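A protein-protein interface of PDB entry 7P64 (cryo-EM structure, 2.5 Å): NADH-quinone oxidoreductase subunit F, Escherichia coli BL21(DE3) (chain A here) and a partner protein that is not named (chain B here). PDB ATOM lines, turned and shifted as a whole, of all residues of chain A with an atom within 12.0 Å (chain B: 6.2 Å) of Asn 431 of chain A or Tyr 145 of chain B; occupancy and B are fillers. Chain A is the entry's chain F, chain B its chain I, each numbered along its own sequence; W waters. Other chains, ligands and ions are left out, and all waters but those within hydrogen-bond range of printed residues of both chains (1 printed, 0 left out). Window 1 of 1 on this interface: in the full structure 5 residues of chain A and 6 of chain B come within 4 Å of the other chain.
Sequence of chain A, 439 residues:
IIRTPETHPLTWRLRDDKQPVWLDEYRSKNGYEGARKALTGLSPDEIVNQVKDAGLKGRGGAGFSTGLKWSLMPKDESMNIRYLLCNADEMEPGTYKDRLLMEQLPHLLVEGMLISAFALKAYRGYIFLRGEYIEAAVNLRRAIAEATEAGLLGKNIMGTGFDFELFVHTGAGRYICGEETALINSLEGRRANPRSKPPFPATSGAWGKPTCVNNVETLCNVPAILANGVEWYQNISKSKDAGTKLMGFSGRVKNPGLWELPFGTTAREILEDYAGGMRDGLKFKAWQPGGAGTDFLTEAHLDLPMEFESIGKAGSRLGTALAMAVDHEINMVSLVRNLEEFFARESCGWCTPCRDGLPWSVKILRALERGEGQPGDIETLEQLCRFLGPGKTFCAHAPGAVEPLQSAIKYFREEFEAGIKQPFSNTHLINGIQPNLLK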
ATOM      1  N   THR A 427      -7.181  13.910 -35.169  1.00  0.00           N
ATOM      2  CA  THR A 427      -6.449  13.545 -33.972  1.00  0.00           C
ATOM      3  C   THR A 427      -5.406  12.493 -34.307  1.00  0.00           C
ATOM      4  O   THR A 427      -5.538  11.745 -35.279  1.00  0.00           O
ATOM      5  CB  THR A 427      -7.386  12.988 -32.891  1.00  0.00           C
ATOM      6  OG1 THR A 427      -7.712  11.630 -33.207  1.00  0.00           O
ATOM      7  CG2 THR A 427      -8.667  13.787 -32.815  1.00  0.00           C
ATOM      8  N   HIS A 428      -4.360  12.443 -33.494  1.00  0.00           N
ATOM      9  CA  HIS A 428      -3.463  11.303 -33.476  1.00  0.00           C
ATOM     10  C   HIS A 428      -3.750  10.470 -32.236  1.00  0.00           C
ATOM     11  O   HIS A 428      -4.340  10.949 -31.265  1.00  0.00           O
ATOM     12  CB  HIS A 428      -1.988  11.733 -33.515  1.00  0.00           C
ATOM     13  CG  HIS A 428      -1.610  12.741 -32.474  1.00  0.00           C
ATOM     14  ND1 HIS A 428      -1.367  12.404 -31.160  1.00  0.00           N
ATOM     15  CD2 HIS A 428      -1.396  14.076 -32.564  1.00  0.00           C
ATOM     16  CE1 HIS A 428      -1.039  13.489 -30.481  1.00  0.00           C
ATOM     17  NE2 HIS A 428      -1.049  14.517 -31.310  1.00  0.00           N
ATOM     18  N   LEU A 429      -3.366   9.200 -32.296  1.00  0.00           N
ATOM     19  CA  LEU A 429      -3.548   8.322 -31.150  1.00  0.00           C
ATOM     20  C   LEU A 429      -2.617   8.732 -30.019  1.00  0.00           C
ATOM     21  O   LEU A 429      -1.443   9.042 -30.239  1.00  0.00           O
ATOM     22  CB  LEU A 429      -3.287   6.868 -31.538  1.00  0.00           C
ATOM     23  CG  LEU A 429      -4.336   6.168 -32.403  1.00  0.00           C
ATOM     24  CD1 LEU A 429      -3.957   4.712 -32.608  1.00  0.00           C
ATOM     25  CD2 LEU A 429      -5.717   6.280 -31.786  1.00  0.00           C
ATOM     26  N   ILE A 430      -3.150   8.742 -28.805  1.00  0.00           N
ATOM     27  CA  ILE A 430      -2.375   9.002 -27.601  1.00  0.00           C
ATOM     28  C   ILE A 430      -2.319   7.703 -26.816  1.00  0.00           C
ATOM     29  O   ILE A 430      -3.362   7.132 -26.476  1.00  0.00           O
ATOM     30  CB  ILE A 430      -2.980  10.143 -26.770  1.00  0.00           C
ATOM     31  CG1 ILE A 430      -2.748  11.478 -27.476  1.00  0.00           C
ATOM     32  CG2 ILE A 430      -2.376  10.176 -25.378  1.00  0.00           C
ATOM     33  CD1 ILE A 430      -3.699  12.551 -27.065  1.00  0.00           C
ATOM     34  N   ASN A 431      -1.104   7.232 -26.547  1.00  0.00           N
ATOM     35  CA  ASN A 431      -0.907   5.932 -25.922  1.00  0.00           C
ATOM     36  C   ASN A 431      -1.380   5.966 -24.474  1.00  0.00           C
ATOM     37  O   ASN A 431      -0.924   6.797 -23.683  1.00  0.00           O
ATOM     38  CB  ASN A 431       0.565   5.539 -26.004  1.00  0.00           C
ATOM     39  CG  ASN A 431       0.783   4.053 -25.839  1.00  0.00           C
ATOM     40  OD1 ASN A 431      -0.150   3.303 -25.566  1.00  0.00           O
ATOM     41  ND2 ASN A 431       2.023   3.618 -26.010  1.00  0.00           N
ATOM     42  N   GLY A 432      -2.283   5.055 -24.128  1.00  0.00           N
ATOM     43  CA  GLY A 432      -2.860   4.997 -22.806  1.00  0.00           C
ATOM     44  C   GLY A 432      -4.264   5.546 -22.699  1.00  0.00           C
ATOM     45  O   GLY A 432      -4.910   5.347 -21.666  1.00  0.00           O
ATOM     46  N   ILE A 433      -4.758   6.225 -23.729  1.00  0.00           N
ATOM     47  CA  ILE A 433      -6.098   6.794 -23.727  1.00  0.00           C
ATOM     48  C   ILE A 433      -6.868   6.195 -24.893  1.00  0.00           C
ATOM     49  O   ILE A 433      -6.470   6.354 -26.054  1.00  0.00           O
ATOM     50  CB  ILE A 433      -6.068   8.327 -23.819  1.00  0.00           C
ATOM     51  CG1 ILE A 433      -5.401   8.911 -22.577  1.00  0.00           C
ATOM     52  CG2 ILE A 433      -7.472   8.878 -23.976  1.00  0.00           C
ATOM     53  CD1 ILE A 433      -5.060  10.358 -22.698  1.00  0.00           C
ATOM     54  N   GLN A 434      -7.955   5.511 -24.589  1.00  0.00           N
ATOM     55  CA  GLN A 434      -8.808   4.961 -25.631  1.00  0.00           C
ATOM     56  C   GLN A 434      -9.694   6.061 -26.203  1.00  0.00           C
ATOM     57  O   GLN A 434     -10.365   6.764 -25.442  1.00  0.00           O
ATOM     58  CB  GLN A 434      -9.663   3.831 -25.084  1.00  0.00           C
ATOM     59  CG  GLN A 434      -8.890   2.566 -24.790  1.00  0.00           C
ATOM     60  CD  GLN A 434      -9.657   1.624 -23.896  1.00  0.00           C
ATOM     61  OE1 GLN A 434      -9.850   1.896 -22.716  1.00  0.00           O
ATOM     62  NE2 GLN A 434     -10.102   0.508 -24.453  1.00  0.00           N
ATOM     63  N   PRO A 435      -9.710   6.250 -27.519  1.00  0.00           N
ATOM     64  CA  PRO A 435     -10.522   7.321 -28.101  1.00  0.00           C
ATOM     65  C   PRO A 435     -12.012   7.041 -27.992  1.00  0.00           C
ATOM     66  O   PRO A 435     -12.453   5.895 -27.894  1.00  0.00           O
ATOM     67  CB  PRO A 435     -10.072   7.348 -29.564  1.00  0.00           C
ATOM     68  CG  PRO A 435      -9.594   5.970 -29.825  1.00  0.00           C
ATOM     69  CD  PRO A 435      -8.978   5.491 -28.545  1.00  0.00           C
ATOM     70  N   ASN A 436     -12.789   8.120 -28.001  1.00  0.00           N
ATOM     71  CA  ASN A 436     -14.243   8.031 -28.071  1.00  0.00           C
ATOM     72  C   ASN A 436     -14.621   7.757 -29.519  1.00  0.00           C
ATOM     73  O   ASN A 436     -14.682   8.670 -30.343  1.00  0.00           O
ATOM     74  CB  ASN A 436     -14.886   9.313 -27.559  1.00  0.00           C
ATOM     75  CG  ASN A 436     -16.293   9.097 -27.063  1.00  0.00           C
ATOM     76  OD1 ASN A 436     -16.625   8.027 -26.567  1.00  0.00           O
ATOM     77  ND2 ASN A 436     -17.132  10.114 -27.201  1.00  0.00           N
ATOM     78  N   THR B  51       4.380  12.657 -12.853  1.00  0.00           N
ATOM     79  CA  THR B  51       5.224  11.983 -13.824  1.00  0.00           C
ATOM     80  C   THR B  51       6.048  12.993 -14.617  1.00  0.00           C
ATOM     81  O   THR B  51       5.933  14.207 -14.442  1.00  0.00           O
ATOM     82  CB  THR B  51       4.378  11.116 -14.754  1.00  0.00           C
ATOM     83  OG1 THR B  51       3.397  11.928 -15.405  1.00  0.00           O
ATOM     84  CG2 THR B  51       3.683  10.032 -13.961  1.00  0.00           C
ATOM     85  N   ARG B  52       6.885  12.465 -15.503  1.00  0.00           N
ATOM     86  CA  ARG B  52       7.777  13.259 -16.330  1.00  0.00           C
ATOM     87  C   ARG B  52       7.490  13.003 -17.801  1.00  0.00           C
ATOM     88  O   ARG B  52       7.011  11.936 -18.178  1.00  0.00           O
ATOM     89  CB  ARG B  52       9.241  12.934 -16.034  1.00  0.00           C
ATOM     90  CG  ARG B  52       9.686  13.314 -14.650  1.00  0.00           C
ATOM     91  CD  ARG B  52      11.129  12.937 -14.419  1.00  0.00           C
ATOM     92  NE  ARG B  52      11.554  13.243 -13.061  1.00  0.00           N
ATOM     93  CZ  ARG B  52      12.060  14.405 -12.681  1.00  0.00           C
ATOM     94  NH1 ARG B  52      12.220  15.401 -13.534  1.00  0.00           N
ATOM     95  NH2 ARG B  52      12.416  14.574 -11.411  1.00  0.00           N
ATOM     96  N   PRO B  54       8.708  12.457 -21.827  1.00  0.00           N
ATOM     97  CA  PRO B  54       9.809  11.633 -22.367  1.00  0.00           C
ATOM     98  C   PRO B  54      11.155  12.339 -22.465  1.00  0.00           C
ATOM     99  O   PRO B  54      12.187  11.657 -22.473  1.00  0.00           O
ATOM    100  CB  PRO B  54       9.291  11.234 -23.751  1.00  0.00           C
ATOM    101  CG  PRO B  54       7.832  11.176 -23.582  1.00  0.00           C
ATOM    102  CD  PRO B  54       7.471  12.259 -22.610  1.00  0.00           C
ATOM    103  N   ARG B  59       6.057  16.885 -15.964  1.00  0.00           N
ATOM    104  CA  ARG B  59       4.934  17.216 -16.826  1.00  0.00           C
ATOM    105  C   ARG B  59       4.029  18.287 -16.244  1.00  0.00           C
ATOM    106  O   ARG B  59       3.295  18.927 -17.002  1.00  0.00           O
ATOM    107  CB  ARG B  59       4.114  15.963 -17.123  1.00  0.00           C
ATOM    108  CG  ARG B  59       4.719  15.110 -18.200  1.00  0.00           C
ATOM    109  CD  ARG B  59       3.694  14.318 -18.961  1.00  0.00           C
ATOM    110  NE  ARG B  59       3.502  12.991 -18.401  1.00  0.00           N
ATOM    111  CZ  ARG B  59       3.507  11.873 -19.108  1.00  0.00           C
ATOM    112  NH1 ARG B  59       3.719  11.881 -20.412  1.00  0.00           N
ATOM    113  NH2 ARG B  59       3.289  10.718 -18.491  1.00  0.00           N
ATOM    114  N   GLU B 106      -6.656  13.156 -11.748  1.00  0.00           N
ATOM    115  CA  GLU B 106      -6.032  12.590 -12.941  1.00  0.00           C
ATOM    116  C   GLU B 106      -6.903  12.816 -14.168  1.00  0.00           C
ATOM    117  O   GLU B 106      -6.393  13.093 -15.257  1.00  0.00           O
ATOM    118  CB  GLU B 106      -5.759  11.099 -12.739  1.00  0.00           C
ATOM    119  CG  GLU B 106      -5.217  10.402 -13.978  1.00  0.00           C
ATOM    120  CD  GLU B 106      -5.053   8.908 -13.813  1.00  0.00           C
ATOM    121  OE1 GLU B 106      -5.119   8.412 -12.673  1.00  0.00           O
ATOM    122  OE2 GLU B 106      -4.860   8.225 -14.837  1.00  0.00           O
ATOM    123  N   THR B 112      -1.409  15.080 -18.322  1.00  0.00           N
ATOM    124  CA  THR B 112      -1.178  13.722 -17.810  1.00  0.00           C
ATOM    125  C   THR B 112      -0.051  13.675 -16.782  1.00  0.00           C
ATOM    126  O   THR B 112       0.633  12.661 -16.644  1.00  0.00           O
ATOM    127  CB  THR B 112      -0.912  12.703 -18.929  1.00  0.00           C
ATOM    128  OG1 THR B 112       0.396  12.909 -19.471  1.00  0.00           O
ATOM    129  CG2 THR B 112      -1.938  12.827 -20.034  1.00  0.00           C
ATOM    130  N   ILE B 114      -0.375  14.290 -13.205  1.00  0.00           N
ATOM    131  CA  ILE B 114      -0.833  13.603 -12.007  1.00  0.00           C
ATOM    132  C   ILE B 114      -1.517  12.306 -12.420  1.00  0.00           C
ATOM    133  O   ILE B 114      -2.307  12.274 -13.371  1.00  0.00           O
ATOM    134  CB  ILE B 114      -1.741  14.522 -11.166  1.00  0.00           C
ATOM    135  CG1 ILE B 114      -2.096  13.886  -9.838  1.00  0.00           C
ATOM    136  CG2 ILE B 114      -3.003  14.938 -11.887  1.00  0.00           C
ATOM    137  CD1 ILE B 114      -2.511  14.885  -8.787  1.00  0.00           C
ATOM    138  N   GLN B 115      -1.147  11.213 -11.764  1.00  0.00           N
ATOM    139  CA  GLN B 115      -1.666   9.901 -12.116  1.00  0.00           C
ATOM    140  C   GLN B 115      -1.910   9.101 -10.850  1.00  0.00           C
ATOM    141  O   GLN B 115      -1.199   9.248  -9.856  1.00  0.00           O
ATOM    142  CB  GLN B 115      -0.705   9.129 -13.029  1.00  0.00           C
ATOM    143  CG  GLN B 115      -0.591   9.664 -14.443  1.00  0.00           C
ATOM    144  CD  GLN B 115       0.538   9.024 -15.208  1.00  0.00           C
ATOM    145  OE1 GLN B 115       0.950   7.911 -14.906  1.00  0.00           O
ATOM    146  NE2 GLN B 115       1.056   9.730 -16.200  1.00  0.00           N
ATOM    147  N   PRO B 142       7.369   8.441 -17.237  1.00  0.00           N
ATOM    148  CA  PRO B 142       6.052   8.926 -17.664  1.00  0.00           C
ATOM    149  C   PRO B 142       4.846   8.213 -17.075  1.00  0.00           C
ATOM    150  O   PRO B 142       3.726   8.707 -17.256  1.00  0.00           O
ATOM    151  CB  PRO B 142       6.107   8.727 -19.183  1.00  0.00           C
ATOM    152  CG  PRO B 142       6.989   7.560 -19.363  1.00  0.00           C
ATOM    153  CD  PRO B 142       8.011   7.607 -18.268  1.00  0.00           C
ATOM    154  N   GLY B 143       5.023   7.091 -16.393  1.00  0.00           N
ATOM    155  CA  GLY B 143       3.879   6.426 -15.789  1.00  0.00           C
ATOM    156  C   GLY B 143       3.009   5.745 -16.827  1.00  0.00           C
ATOM    157  O   GLY B 143       3.499   5.043 -17.717  1.00  0.00           O
ATOM    158  N   LYS B 144       1.698   5.955 -16.720  1.00  0.00           N
ATOM    159  CA  LYS B 144       0.721   5.249 -17.539  1.00  0.00           C
ATOM    160  C   LYS B 144       0.561   5.829 -18.937  1.00  0.00           C
ATOM    161  O   LYS B 144      -0.030   5.168 -19.794  1.00  0.00           O
ATOM    162  CB  LYS B 144      -0.641   5.244 -16.843  1.00  0.00           C
ATOM    163  CG  LYS B 144      -0.631   4.607 -15.472  1.00  0.00           C
ATOM    164  CD  LYS B 144      -2.041   4.384 -14.958  1.00  0.00           C
ATOM    165  CE  LYS B 144      -2.745   5.698 -14.696  1.00  0.00           C
ATOM    166  NZ  LYS B 144      -4.047   5.497 -14.004  1.00  0.00           N
ATOM    167  N   TYR B 145       1.055   7.040 -19.190  1.00  0.00           N
ATOM    168  CA  TYR B 145       0.937   7.697 -20.491  1.00  0.00           C
ATOM    169  C   TYR B 145       2.347   7.965 -20.992  1.00  0.00           C
ATOM    170  O   TYR B 145       2.944   9.005 -20.676  1.00  0.00           O
ATOM    171  CB  TYR B 145       0.114   8.977 -20.385  1.00  0.00           C
ATOM    172  CG  TYR B 145      -1.195   8.775 -19.663  1.00  0.00           C
ATOM    173  CD1 TYR B 145      -2.291   8.229 -20.314  1.00  0.00           C
ATOM    174  CD2 TYR B 145      -1.330   9.114 -18.325  1.00  0.00           C
ATOM    175  CE1 TYR B 145      -3.485   8.036 -19.654  1.00  0.00           C
ATOM    176  CE2 TYR B 145      -2.518   8.924 -17.657  1.00  0.00           C
ATOM    177  CZ  TYR B 145      -3.592   8.385 -18.327  1.00  0.00           C
ATOM    178  OH  TYR B 145      -4.780   8.195 -17.662  1.00  0.00           O
ATOM    179  N   PRO B 146       2.918   7.055 -21.786  1.00  0.00           N
ATOM    180  CA  PRO B 146       4.368   7.067 -22.007  1.00  0.00           C
ATOM    181  C   PRO B 146       4.880   8.121 -22.973  1.00  0.00           C
ATOM    182  O   PRO B 146       6.097   8.335 -23.018  1.00  0.00           O
ATOM    183  CB  PRO B 146       4.639   5.661 -22.556  1.00  0.00           C
ATOM    184  CG  PRO B 146       3.374   5.275 -23.213  1.00  0.00           C
ATOM    185  CD  PRO B 146       2.270   5.894 -22.416  1.00  0.00           C
ATOM    186  N   GLU B 147       4.025   8.789 -23.742  1.00  0.00           N
ATOM    187  CA  GLU B 147       4.524   9.645 -24.809  1.00  0.00           C
ATOM    188  C   GLU B 147       3.941  11.047 -24.854  1.00  0.00           C
ATOM    189  O   GLU B 147       4.493  11.885 -25.572  1.00  0.00           O
ATOM    190  CB  GLU B 147       4.292   8.983 -26.174  1.00  0.00           C
ATOM    191  CG  GLU B 147       5.387   8.018 -26.578  1.00  0.00           C
ATOM    192  CD  GLU B 147       4.843   6.701 -27.087  1.00  0.00           C
ATOM    193  OE1 GLU B 147       3.951   6.722 -27.961  1.00  0.00           O
ATOM    194  OE2 GLU B 147       5.306   5.643 -26.614  1.00  0.00           O
ATOM    195  N   TYR B 148       2.860  11.337 -24.133  1.00  0.00           N
ATOM    196  CA  TYR B 148       2.229  12.642 -24.265  1.00  0.00           C
ATOM    197  C   TYR B 148       3.084  13.731 -23.633  1.00  0.00           C
ATOM    198  O   TYR B 148       3.606  13.577 -22.528  1.00  0.00           O
ATOM    199  CB  TYR B 148       0.840  12.658 -23.635  1.00  0.00           C
ATOM    200  CG  TYR B 148       0.134  13.974 -23.871  1.00  0.00           C
ATOM    201  CD1 TYR B 148      -0.375  14.291 -25.123  1.00  0.00           C
ATOM    202  CD2 TYR B 148       0.010  14.914 -22.856  1.00  0.00           C
ATOM    203  CE1 TYR B 148      -1.003  15.493 -25.352  1.00  0.00           C
ATOM    204  CE2 TYR B 148      -0.617  16.121 -23.078  1.00  0.00           C
ATOM    205  CZ  TYR B 148      -1.124  16.403 -24.327  1.00  0.00           C
ATOM    206  OH  TYR B 148      -1.751  17.601 -24.557  1.00  0.00           O
HETATM  207  O   HOH W   1       1.000   8.923 -24.177  1.00  0.00           O
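Printed residues of chain A that touch a printed residue of chain B: Asn 431, Gly 432 and Ile 433. Hydrophobic or aromatic side chains of chain A within 4 Å of the printed part of chain B: Ile 433. Of the 15 printed residues of chain B, 3 touch a printed residue of chain A. Hydrophobic or aromatic side chains of chain B that line the printed part of chain A: Tyr 145 and Pro 146. Among the printed residues, 5 pairs touch across the chains. Among the printed residues, no Asp or Glu carboxylate lies within 4 Å of a Lys or Arg side-chain nitrogen of the other chain.
Tyr 145 of chain B touches Asn 431 of chain A. ND2 of Asn 431 of chain A touches CG of Pro 146 of chain B, at 3.5 Å. ND2 of Asn 431 of chain A touches OE2 of Glu 147 of chain B, at 3.9 Å. Gly 432 of chain A touches Tyr 145 of chain B. Ile 433 of chain A touches Tyr 145 of chain B.
Water W1 lies within hydrogen-bond range of the backbone carbonyl oxygen (O) of Asn 431 of chain A (2.9 Å), the backbone NH (N) of Tyr 148 of chain B (3.0 Å) and the backbone NH (N) of Glu 147 of chain B (3.1 Å).
The guanidinium group (NH2) of Arg 59 of chain B is in hydrogen-bond range of the backbone carbonyl oxygen (O) of Tyr 145 of chain B (2.8 Å). OE2 of Glu 106 of chain B lies within hydrogen-bond range of OH of Tyr 145 of chain B (2.8 Å).
Leu 429 of chain A touches none of the printed residues of chain B. Asn 431 of chain A touches just these residues of chain B: Tyr 145 (3.8 Å), Pro 146 (3.5 Å) and Glu 147 (3.9 Å). Printed residues of chain B within 4 Å of Gly 432 of chain A: Tyr 145 (3.6 Å). Printed residues of chain B within 4 Å of Ile 433 of chain A: Tyr 145. Asn 436 of chain A touches none of the printed residues of chain B. Glu 106 of chain B touches none of the printed residues of chain A. Thr 112 of chain B touches none of the printed residues of chain A. No residue of chain A comes within 4 Å of Gln 115 of chain B. No residue of chain A comes within 4 Å of Pro 142 of chain B. Gly 143 of chain B touches none of the printed residues of chain A. No residue of chain A comes within 4 Å of Lys 144 of chain B. Printed residues of chain A within 4 Å of Tyr 145 of chain B: Asn 431, Gly 432 and Ile 433. Of chain A, only Asn 431 comes within 4 Å of Pro 146 of chain B. Glu 147 of chain B touches just one residue of chain A: Asn 431 (3.9 Å). The nearest residue of chain B that does not touch Asn 431 of chain A is Lys 144 of chain B (4.3 Å). The nearest residue of chain A that does not touch Tyr 145 of chain B is Ile 430 of chain A (5.4 Å). The nearest printed residue of chain B that does not touch Ile 433 of chain A is Thr 112 of chain B (4.8 Å).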
